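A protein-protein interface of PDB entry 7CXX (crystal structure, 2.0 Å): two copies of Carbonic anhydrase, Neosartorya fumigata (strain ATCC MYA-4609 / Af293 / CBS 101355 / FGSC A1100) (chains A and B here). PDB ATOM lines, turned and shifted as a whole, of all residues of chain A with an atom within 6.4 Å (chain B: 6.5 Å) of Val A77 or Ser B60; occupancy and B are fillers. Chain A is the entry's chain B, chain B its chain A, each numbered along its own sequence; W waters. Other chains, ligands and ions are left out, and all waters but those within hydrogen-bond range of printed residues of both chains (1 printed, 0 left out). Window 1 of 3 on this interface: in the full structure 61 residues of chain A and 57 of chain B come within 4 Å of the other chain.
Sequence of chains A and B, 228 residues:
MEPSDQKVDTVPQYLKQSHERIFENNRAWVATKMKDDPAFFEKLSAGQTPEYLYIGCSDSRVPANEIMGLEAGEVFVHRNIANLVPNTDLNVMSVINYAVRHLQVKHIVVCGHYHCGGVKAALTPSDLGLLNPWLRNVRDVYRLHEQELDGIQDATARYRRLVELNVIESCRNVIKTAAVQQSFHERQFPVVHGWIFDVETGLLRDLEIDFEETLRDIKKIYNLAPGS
A ring nitrogen (ND1) of His A78 is in hydrogen-bond range of the backbone carbonyl oxygen (O) of Arg B79, at 2.7 Å.
O of Ala A72 sits close to O of Arg B61 (3.3 Å).
OG of Ser B58 is in hydrogen-bond range of O of Val A77.
The guanidinium group (NH1) of Arg B79 sits at hydrogen-bond distance from the backbone carbonyl oxygen (O) of Cys B57 (2.9 Å).
The backbone carbonyl oxygen of Tyr A52 lies within hydrogen-bond range of the backbone NH of Phe A76 (2.8 Å).
The backbone NH (N) of Gly A56 is in hydrogen-bond range of the backbone carbonyl oxygen (O) of His A78, 3.0 Å away.
O of Asp B59 lies within hydrogen-bond range of NE2 of His B113, at 2.9 Å.
SG of Cys B57 is disulfide-bonded to SG of Cys B116.
The backbone NH (N) of Ser B58 is in hydrogen-bond range of the backbone carbonyl oxygen (O) of Asn B80 (3.1 Å).
Val A75 touches Ser B60 (O to OG, 3.7 Å).
CD1 of Phe A76 touches O of Ser B58, 3.4 Å away.
CE1 of Phe A76 touches N of Asp B59 (3.7 Å).
CG2 of Val A77 touches OG of Ser B60, 3.8 Å away.
Val A77 touches Arg B79.
Leu A53 touches none of the printed residues of chain B.
Printed residues of chain B within 4 Å of Phe A76: Ser B58 (3.4 Å) and Asp B59 (3.7 Å).
Of chain B, only Ser B58 (2.8 Å), Ser B60 (3.8 Å) and Arg B79 (3.5 Å) come within 4 Å of Val A77.
Val A95 touches none of the printed residues of chain B.
Of the printed residues of chain A, Arg B61 touches Ala A72 (3.3 Å).
The nearest residue of chain B that does not touch Val A77 is Cys B57 (5.0 Å).
The nearest residue of chain A that does not touch Ser B60 is Gly A73 (4.4 Å).
Among the printed residues, no Asp or Glu carboxylate lies within 4 Å of a Lys or Arg side-chain nitrogen of the other chain.
1 position is printed for both chains.
Of the 8 pairs that touch across the chains among the printed residues, none has its exchanged pair printed and touching as well.
Water W1 bridges O of Ser B60 and O of Val A75.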
ATOM      1  N   TYR A  52      -3.118   7.979  -6.341  1.00  0.00           N
ATOM      2  CA  TYR A  52      -2.932   7.726  -7.779  1.00  0.00           C
ATOM      3  C   TYR A  52      -2.080   6.461  -7.968  1.00  0.00           C
ATOM      4  O   TYR A  52      -1.055   6.322  -7.264  1.00  0.00           O
ATOM      5  CB  TYR A  52      -2.253   8.924  -8.435  1.00  0.00           C
ATOM      6  CG  TYR A  52      -3.171  10.109  -8.583  1.00  0.00           C
ATOM      7  CD1 TYR A  52      -3.533  10.880  -7.479  1.00  0.00           C
ATOM      8  CD2 TYR A  52      -3.692  10.443  -9.823  1.00  0.00           C
ATOM      9  CE1 TYR A  52      -4.412  11.944  -7.604  1.00  0.00           C
ATOM     10  CE2 TYR A  52      -4.561  11.514  -9.967  1.00  0.00           C
ATOM     11  CZ  TYR A  52      -4.921  12.263  -8.856  1.00  0.00           C
ATOM     12  OH  TYR A  52      -5.772  13.320  -9.007  1.00  0.00           O
ATOM     13  N   LEU A  53      -2.475   5.605  -8.909  1.00  0.00           N
ATOM     14  CA  LEU A  53      -1.519   4.720  -9.640  1.00  0.00           C
ATOM     15  C   LEU A  53      -1.251   5.326 -10.990  1.00  0.00           C
ATOM     16  O   LEU A  53      -2.223   5.618 -11.738  1.00  0.00           O
ATOM     17  CB  LEU A  53      -2.137   3.320  -9.807  1.00  0.00           C
ATOM     18  CG  LEU A  53      -1.454   2.427 -10.837  1.00  0.00           C
ATOM     19  CD1 LEU A  53      -0.041   2.073 -10.351  1.00  0.00           C
ATOM     20  CD2 LEU A  53      -2.266   1.139 -11.036  1.00  0.00           C
ATOM     21  N   TYR A  54       0.023   5.403 -11.338  1.00  0.00           N
ATOM     22  CA  TYR A  54       0.531   5.949 -12.593  1.00  0.00           C
ATOM     23  C   TYR A  54       1.298   4.842 -13.309  1.00  0.00           C
ATOM     24  O   TYR A  54       2.237   4.256 -12.698  1.00  0.00           O
ATOM     25  CB  TYR A  54       1.405   7.162 -12.260  1.00  0.00           C
ATOM     26  CG  TYR A  54       2.054   7.827 -13.440  1.00  0.00           C
ATOM     27  CD1 TYR A  54       3.231   7.336 -13.974  1.00  0.00           C
ATOM     28  CD2 TYR A  54       1.521   8.980 -13.988  1.00  0.00           C
ATOM     29  CE1 TYR A  54       3.832   7.948 -15.053  1.00  0.00           C
ATOM     30  CE2 TYR A  54       2.130   9.628 -15.043  1.00  0.00           C
ATOM     31  CZ  TYR A  54       3.296   9.119 -15.566  1.00  0.00           C
ATOM     32  OH  TYR A  54       3.905   9.782 -16.585  1.00  0.00           O
ATOM     33  N   ILE A  55       0.861   4.531 -14.531  1.00  0.00           N
ATOM     34  CA  ILE A  55       1.487   3.527 -15.412  1.00  0.00           C
ATOM     35  C   ILE A  55       2.088   4.339 -16.541  1.00  0.00           C
ATOM     36  O   ILE A  55       1.314   4.953 -17.265  1.00  0.00           O
ATOM     37  CB  ILE A  55       0.468   2.479 -15.898  1.00  0.00           C
ATOM     38  CG1 ILE A  55      -0.179   1.755 -14.721  1.00  0.00           C
ATOM     39  CG2 ILE A  55       1.126   1.557 -16.909  1.00  0.00           C
ATOM     40  CD1 ILE A  55      -1.362   0.880 -15.070  1.00  0.00           C
ATOM     41  N   GLY A  56       3.416   4.322 -16.658  1.00  0.00           N
ATOM     42  CA  GLY A  56       4.135   5.051 -17.697  1.00  0.00           C
ATOM     43  C   GLY A  56       5.152   4.181 -18.363  1.00  0.00           C
ATOM     44  O   GLY A  56       5.167   2.975 -18.085  1.00  0.00           O
ATOM     45  N   ALA A  64       6.708  11.374 -12.153  1.00  0.00           N
ATOM     46  CA  ALA A  64       5.237  11.508 -12.247  1.00  0.00           C
ATOM     47  C   ALA A  64       4.742  12.597 -11.286  1.00  0.00           C
ATOM     48  O   ALA A  64       3.937  13.458 -11.705  1.00  0.00           O
ATOM     49  CB  ALA A  64       4.569  10.191 -11.942  1.00  0.00           C
ATOM     50  N   ALA A  72       5.818  12.915  -3.891  1.00  0.00           N
ATOM     51  CA  ALA A  72       6.224  11.525  -4.183  1.00  0.00           C
ATOM     52  C   ALA A  72       5.891  10.698  -2.940  1.00  0.00           C
ATOM     53  O   ALA A  72       6.557  10.888  -1.905  1.00  0.00           O
ATOM     54  CB  ALA A  72       7.688  11.462  -4.537  1.00  0.00           C
ATOM     55  N   GLY A  73       4.892   9.830  -3.044  1.00  0.00           N
ATOM     56  CA  GLY A  73       4.211   9.206  -1.898  1.00  0.00           C
ATOM     57  C   GLY A  73       2.709   9.280  -2.111  1.00  0.00           C
ATOM     58  O   GLY A  73       1.988   8.431  -1.544  1.00  0.00           O
ATOM     59  N   VAL A  75       1.718   9.083  -5.262  1.00  0.00           N
ATOM     60  CA  VAL A  75       1.699   8.367  -6.571  1.00  0.00           C
ATOM     61  C   VAL A  75       2.415   7.013  -6.437  1.00  0.00           C
ATOM     62  O   VAL A  75       3.651   7.001  -6.320  1.00  0.00           O
ATOM     63  CB  VAL A  75       2.301   9.218  -7.701  1.00  0.00           C
ATOM     64  CG1 VAL A  75       2.006   8.618  -9.074  1.00  0.00           C
ATOM     65  CG2 VAL A  75       1.819  10.654  -7.661  1.00  0.00           C
ATOM     66  N   PHE A  76       1.646   5.923  -6.484  1.00  0.00           N
ATOM     67  CA  PHE A  76       2.111   4.513  -6.634  1.00  0.00           C
ATOM     68  C   PHE A  76       2.469   4.280  -8.095  1.00  0.00           C
ATOM     69  O   PHE A  76       1.676   4.722  -9.013  1.00  0.00           O
ATOM     70  CB  PHE A  76       1.005   3.585  -6.160  1.00  0.00           C
ATOM     71  CG  PHE A  76       1.400   2.155  -5.918  1.00  0.00           C
ATOM     72  CD1 PHE A  76       2.134   1.797  -4.788  1.00  0.00           C
ATOM     73  CD2 PHE A  76       0.966   1.162  -6.771  1.00  0.00           C
ATOM     74  CE1 PHE A  76       2.446   0.472  -4.537  1.00  0.00           C
ATOM     75  CE2 PHE A  76       1.288  -0.162  -6.535  1.00  0.00           C
ATOM     76  CZ  PHE A  76       2.015  -0.502  -5.411  1.00  0.00           C
ATOM     77  N   VAL A  77       3.626   3.674  -8.383  1.00  0.00           N
ATOM     78  CA  VAL A  77       4.104   3.772  -9.794  1.00  0.00           C
ATOM     79  C   VAL A  77       4.441   2.410 -10.388  1.00  0.00           C
ATOM     80  O   VAL A  77       5.067   1.589  -9.680  1.00  0.00           O
ATOM     81  CB  VAL A  77       5.289   4.729  -9.939  1.00  0.00           C
ATOM     82  CG1 VAL A  77       5.779   4.782 -11.367  1.00  0.00           C
ATOM     83  CG2 VAL A  77       4.937   6.126  -9.455  1.00  0.00           C
ATOM     84  N   HIS A  78       4.110   2.243 -11.681  1.00  0.00           N
ATOM     85  CA  HIS A  78       4.639   1.165 -12.545  1.00  0.00           C
ATOM     86  C   HIS A  78       5.154   1.784 -13.841  1.00  0.00           C
ATOM     87  O   HIS A  78       4.430   2.549 -14.477  1.00  0.00           O
ATOM     88  CB  HIS A  78       3.589   0.112 -12.782  1.00  0.00           C
ATOM     89  CG  HIS A  78       4.030  -0.984 -13.685  1.00  0.00           C
ATOM     90  ND1 HIS A  78       4.923  -1.944 -13.263  1.00  0.00           N
ATOM     91  CD2 HIS A  78       3.635  -1.339 -14.920  1.00  0.00           C
ATOM     92  CE1 HIS A  78       5.095  -2.830 -14.244  1.00  0.00           C
ATOM     93  NE2 HIS A  78       4.291  -2.505 -15.255  1.00  0.00           N
ATOM     94  N   ARG A  79       6.339   1.382 -14.281  1.00  0.00           N
ATOM     95  CA  ARG A  79       6.818   1.707 -15.636  1.00  0.00           C
ATOM     96  C   ARG A  79       7.268   0.435 -16.357  1.00  0.00           C
ATOM     97  O   ARG A  79       7.954  -0.421 -15.706  1.00  0.00           O
ATOM     98  CB  ARG A  79       8.000   2.677 -15.580  1.00  0.00           C
ATOM     99  CG  ARG A  79       7.678   4.017 -14.936  1.00  0.00           C
ATOM    100  CD  ARG A  79       8.911   4.927 -14.869  1.00  0.00           C
ATOM    101  NE  ARG A  79       8.560   6.268 -14.392  1.00  0.00           N
ATOM    102  CZ  ARG A  79       8.039   7.249 -15.142  1.00  0.00           C
ATOM    103  NH1 ARG A  79       7.848   7.073 -16.432  1.00  0.00           N
ATOM    104  NH2 ARG A  79       7.754   8.436 -14.602  1.00  0.00           N
ATOM    105  N   VAL A  95       0.298  -5.008  -9.819  1.00  0.00           N
ATOM    106  CA  VAL A  95       0.308  -3.577  -9.367  1.00  0.00           C
ATOM    107  C   VAL A  95      -1.125  -3.033  -9.357  1.00  0.00           C
ATOM    108  O   VAL A  95      -1.477  -2.378  -8.348  1.00  0.00           O
ATOM    109  CB  VAL A  95       1.323  -2.632 -10.036  1.00  0.00           C
ATOM    110  CG1 VAL A  95       2.528  -3.306 -10.606  1.00  0.00           C
ATOM    111  CG2 VAL A  95       0.739  -1.637 -10.975  1.00  0.00           C
ATOM    112  N   CYS B  57      10.671  -0.782  -6.107  1.00  0.00           N
ATOM    113  CA  CYS B  57       9.292  -1.172  -5.797  1.00  0.00           C
ATOM    114  C   CYS B  57       8.354  -0.032  -6.231  1.00  0.00           C
ATOM    115  O   CYS B  57       8.759   1.105  -6.358  1.00  0.00           O
ATOM    116  CB  CYS B  57       9.171  -1.670  -4.362  1.00  0.00           C
ATOM    117  SG  CYS B  57       9.358  -0.391  -3.094  1.00  0.00           S
ATOM    118  N   SER B  58       7.136  -0.382  -6.580  1.00  0.00           N
ATOM    119  CA  SER B  58       6.040   0.546  -6.969  1.00  0.00           C
ATOM    120  C   SER B  58       5.701   1.463  -5.794  1.00  0.00           C
ATOM    121  O   SER B  58       5.158   2.539  -6.067  1.00  0.00           O
ATOM    122  CB  SER B  58       4.834  -0.243  -7.438  1.00  0.00           C
ATOM    123  OG  SER B  58       5.181  -0.973  -8.606  1.00  0.00           O
ATOM    124  N   ASP B  59       6.063   1.064  -4.570  1.00  0.00           N
ATOM    125  CA  ASP B  59       5.957   1.884  -3.333  1.00  0.00           C
ATOM    126  C   ASP B  59       7.159   2.841  -3.266  1.00  0.00           C
ATOM    127  O   ASP B  59       7.920   2.791  -2.289  1.00  0.00           O
ATOM    128  CB  ASP B  59       5.806   0.968  -2.115  1.00  0.00           C
ATOM    129  CG  ASP B  59       4.627   1.325  -1.218  1.00  0.00           C
ATOM    130  OD1 ASP B  59       4.491   2.518  -0.859  1.00  0.00           O
ATOM    131  OD2 ASP B  59       3.828   0.421  -0.905  1.00  0.00           O
ATOM    132  N   SER B  60       7.315   3.687  -4.290  1.00  0.00           N
ATOM    133  CA  SER B  60       8.354   4.745  -4.430  1.00  0.00           C
ATOM    134  C   SER B  60       8.215   5.805  -3.325  1.00  0.00           C
ATOM    135  O   SER B  60       7.103   6.031  -2.833  1.00  0.00           O
ATOM    136  CB  SER B  60       8.300   5.379  -5.822  1.00  0.00           C
ATOM    137  OG  SER B  60       6.975   5.369  -6.350  1.00  0.00           O
ATOM    138  N   ARG B  61       9.323   6.441  -2.957  1.00  0.00           N
ATOM    139  CA  ARG B  61       9.387   7.522  -1.929  1.00  0.00           C
ATOM    140  C   ARG B  61      10.036   8.774  -2.542  1.00  0.00           C
ATOM    141  O   ARG B  61       9.685   9.912  -2.131  1.00  0.00           O
ATOM    142  CB  ARG B  61      10.220   7.040  -0.731  1.00  0.00           C
ATOM    143  CG  ARG B  61       9.603   5.898   0.064  1.00  0.00           C
ATOM    144  CD  ARG B  61       8.388   6.328   0.876  1.00  0.00           C
ATOM    145  NE  ARG B  61       7.739   5.170   1.474  1.00  0.00           N
ATOM    146  CZ  ARG B  61       6.852   4.379   0.868  1.00  0.00           C
ATOM    147  NH1 ARG B  61       6.340   3.340   1.505  1.00  0.00           N
ATOM    148  NH2 ARG B  61       6.457   4.628  -0.366  1.00  0.00           N
ATOM    149  N   VAL B  62      11.002   8.553  -3.439  1.00  0.00           N
ATOM    150  CA  VAL B  62      11.826   9.601  -4.099  1.00  0.00           C
ATOM    151  C   VAL B  62      12.192   9.066  -5.473  1.00  0.00           C
ATOM    152  O   VAL B  62      12.517   7.889  -5.627  1.00  0.00           O
ATOM    153  CB  VAL B  62      13.106   9.932  -3.309  1.00  0.00           C
ATOM    154  CG1 VAL B  62      13.843  11.105  -3.938  1.00  0.00           C
ATOM    155  CG2 VAL B  62      12.853  10.183  -1.838  1.00  0.00           C
ATOM    156  N   PRO B  63      12.136   9.905  -6.521  1.00  0.00           N
ATOM    157  CA  PRO B  63      12.569   9.456  -7.838  1.00  0.00           C
ATOM    158  C   PRO B  63      13.987   8.868  -7.766  1.00  0.00           C
ATOM    159  O   PRO B  63      14.795   9.380  -7.050  1.00  0.00           O
ATOM    160  CB  PRO B  63      12.486  10.743  -8.675  1.00  0.00           C
ATOM    161  CG  PRO B  63      11.394  11.565  -7.991  1.00  0.00           C
ATOM    162  CD  PRO B  63      11.575  11.271  -6.518  1.00  0.00           C
ATOM    163  N   ARG B  79       9.473  -0.288 -11.978  1.00  0.00           N
ATOM    164  CA  ARG B  79       8.989  -0.524 -10.597  1.00  0.00           C
ATOM    165  C   ARG B  79       7.885  -1.588 -10.620  1.00  0.00           C
ATOM    166  O   ARG B  79       6.942  -1.509 -11.476  1.00  0.00           O
ATOM    167  CB  ARG B  79       8.438   0.756  -9.990  1.00  0.00           C
ATOM    168  CG  ARG B  79       9.505   1.821  -9.820  1.00  0.00           C
ATOM    169  CD  ARG B  79       8.933   3.079  -9.201  1.00  0.00           C
ATOM    170  NE  ARG B  79      10.001   4.059  -9.011  1.00  0.00           N
ATOM    171  CZ  ARG B  79      10.823   4.087  -7.962  1.00  0.00           C
ATOM    172  NH1 ARG B  79      10.693   3.234  -6.961  1.00  0.00           N
ATOM    173  NH2 ARG B  79      11.730   5.042  -7.880  1.00  0.00           N
ATOM    174  N   ASN B  80       7.951  -2.522  -9.683  1.00  0.00           N
ATOM    175  CA  ASN B  80       6.909  -3.572  -9.575  1.00  0.00           C
ATOM    176  C   ASN B  80       6.755  -3.916  -8.097  1.00  0.00           C
ATOM    177  O   ASN B  80       7.545  -3.383  -7.300  1.00  0.00           O
ATOM    178  CB  ASN B  80       7.245  -4.730 -10.518  1.00  0.00           C
ATOM    179  CG  ASN B  80       8.431  -5.565 -10.066  1.00  0.00           C
ATOM    180  OD1 ASN B  80       8.587  -5.792  -8.886  1.00  0.00           O
ATOM    181  ND2 ASN B  80       9.289  -5.952 -10.987  1.00  0.00           N
ATOM    182  N   HIS B 113      13.766  -1.145  -0.125  1.00  0.00           N
ATOM    183  CA  HIS B 113      13.725  -0.432   1.165  1.00  0.00           C
ATOM    184  C   HIS B 113      12.770  -1.161   2.089  1.00  0.00           C
ATOM    185  O   HIS B 113      11.975  -1.949   1.597  1.00  0.00           O
ATOM    186  CB  HIS B 113      13.373   1.040   0.956  1.00  0.00           C
ATOM    187  CG  HIS B 113      12.054   1.306   0.332  1.00  0.00           C
ATOM    188  ND1 HIS B 113      10.888   1.242   1.053  1.00  0.00           N
ATOM    189  CD2 HIS B 113      11.726   1.742  -0.899  1.00  0.00           C
ATOM    190  CE1 HIS B 113       9.880   1.587   0.274  1.00  0.00           C
ATOM    191  NE2 HIS B 113      10.367   1.887  -0.933  1.00  0.00           N
ATOM    192  N   CYS B 116       8.554  -1.238   1.546  1.00  0.00           N
ATOM    193  CA  CYS B 116       7.732  -1.687   0.382  1.00  0.00           C
ATOM    194  C   CYS B 116       6.667  -2.634   0.950  1.00  0.00           C
ATOM    195  O   CYS B 116       7.003  -3.610   1.687  1.00  0.00           O
ATOM    196  CB  CYS B 116       8.467  -2.291  -0.818  1.00  0.00           C
ATOM    197  SG  CYS B 116       9.930  -1.392  -1.406  1.00  0.00           S
HETATM  198  O   HOH W   1       4.956   6.203  -4.007  1.00  0.00           O
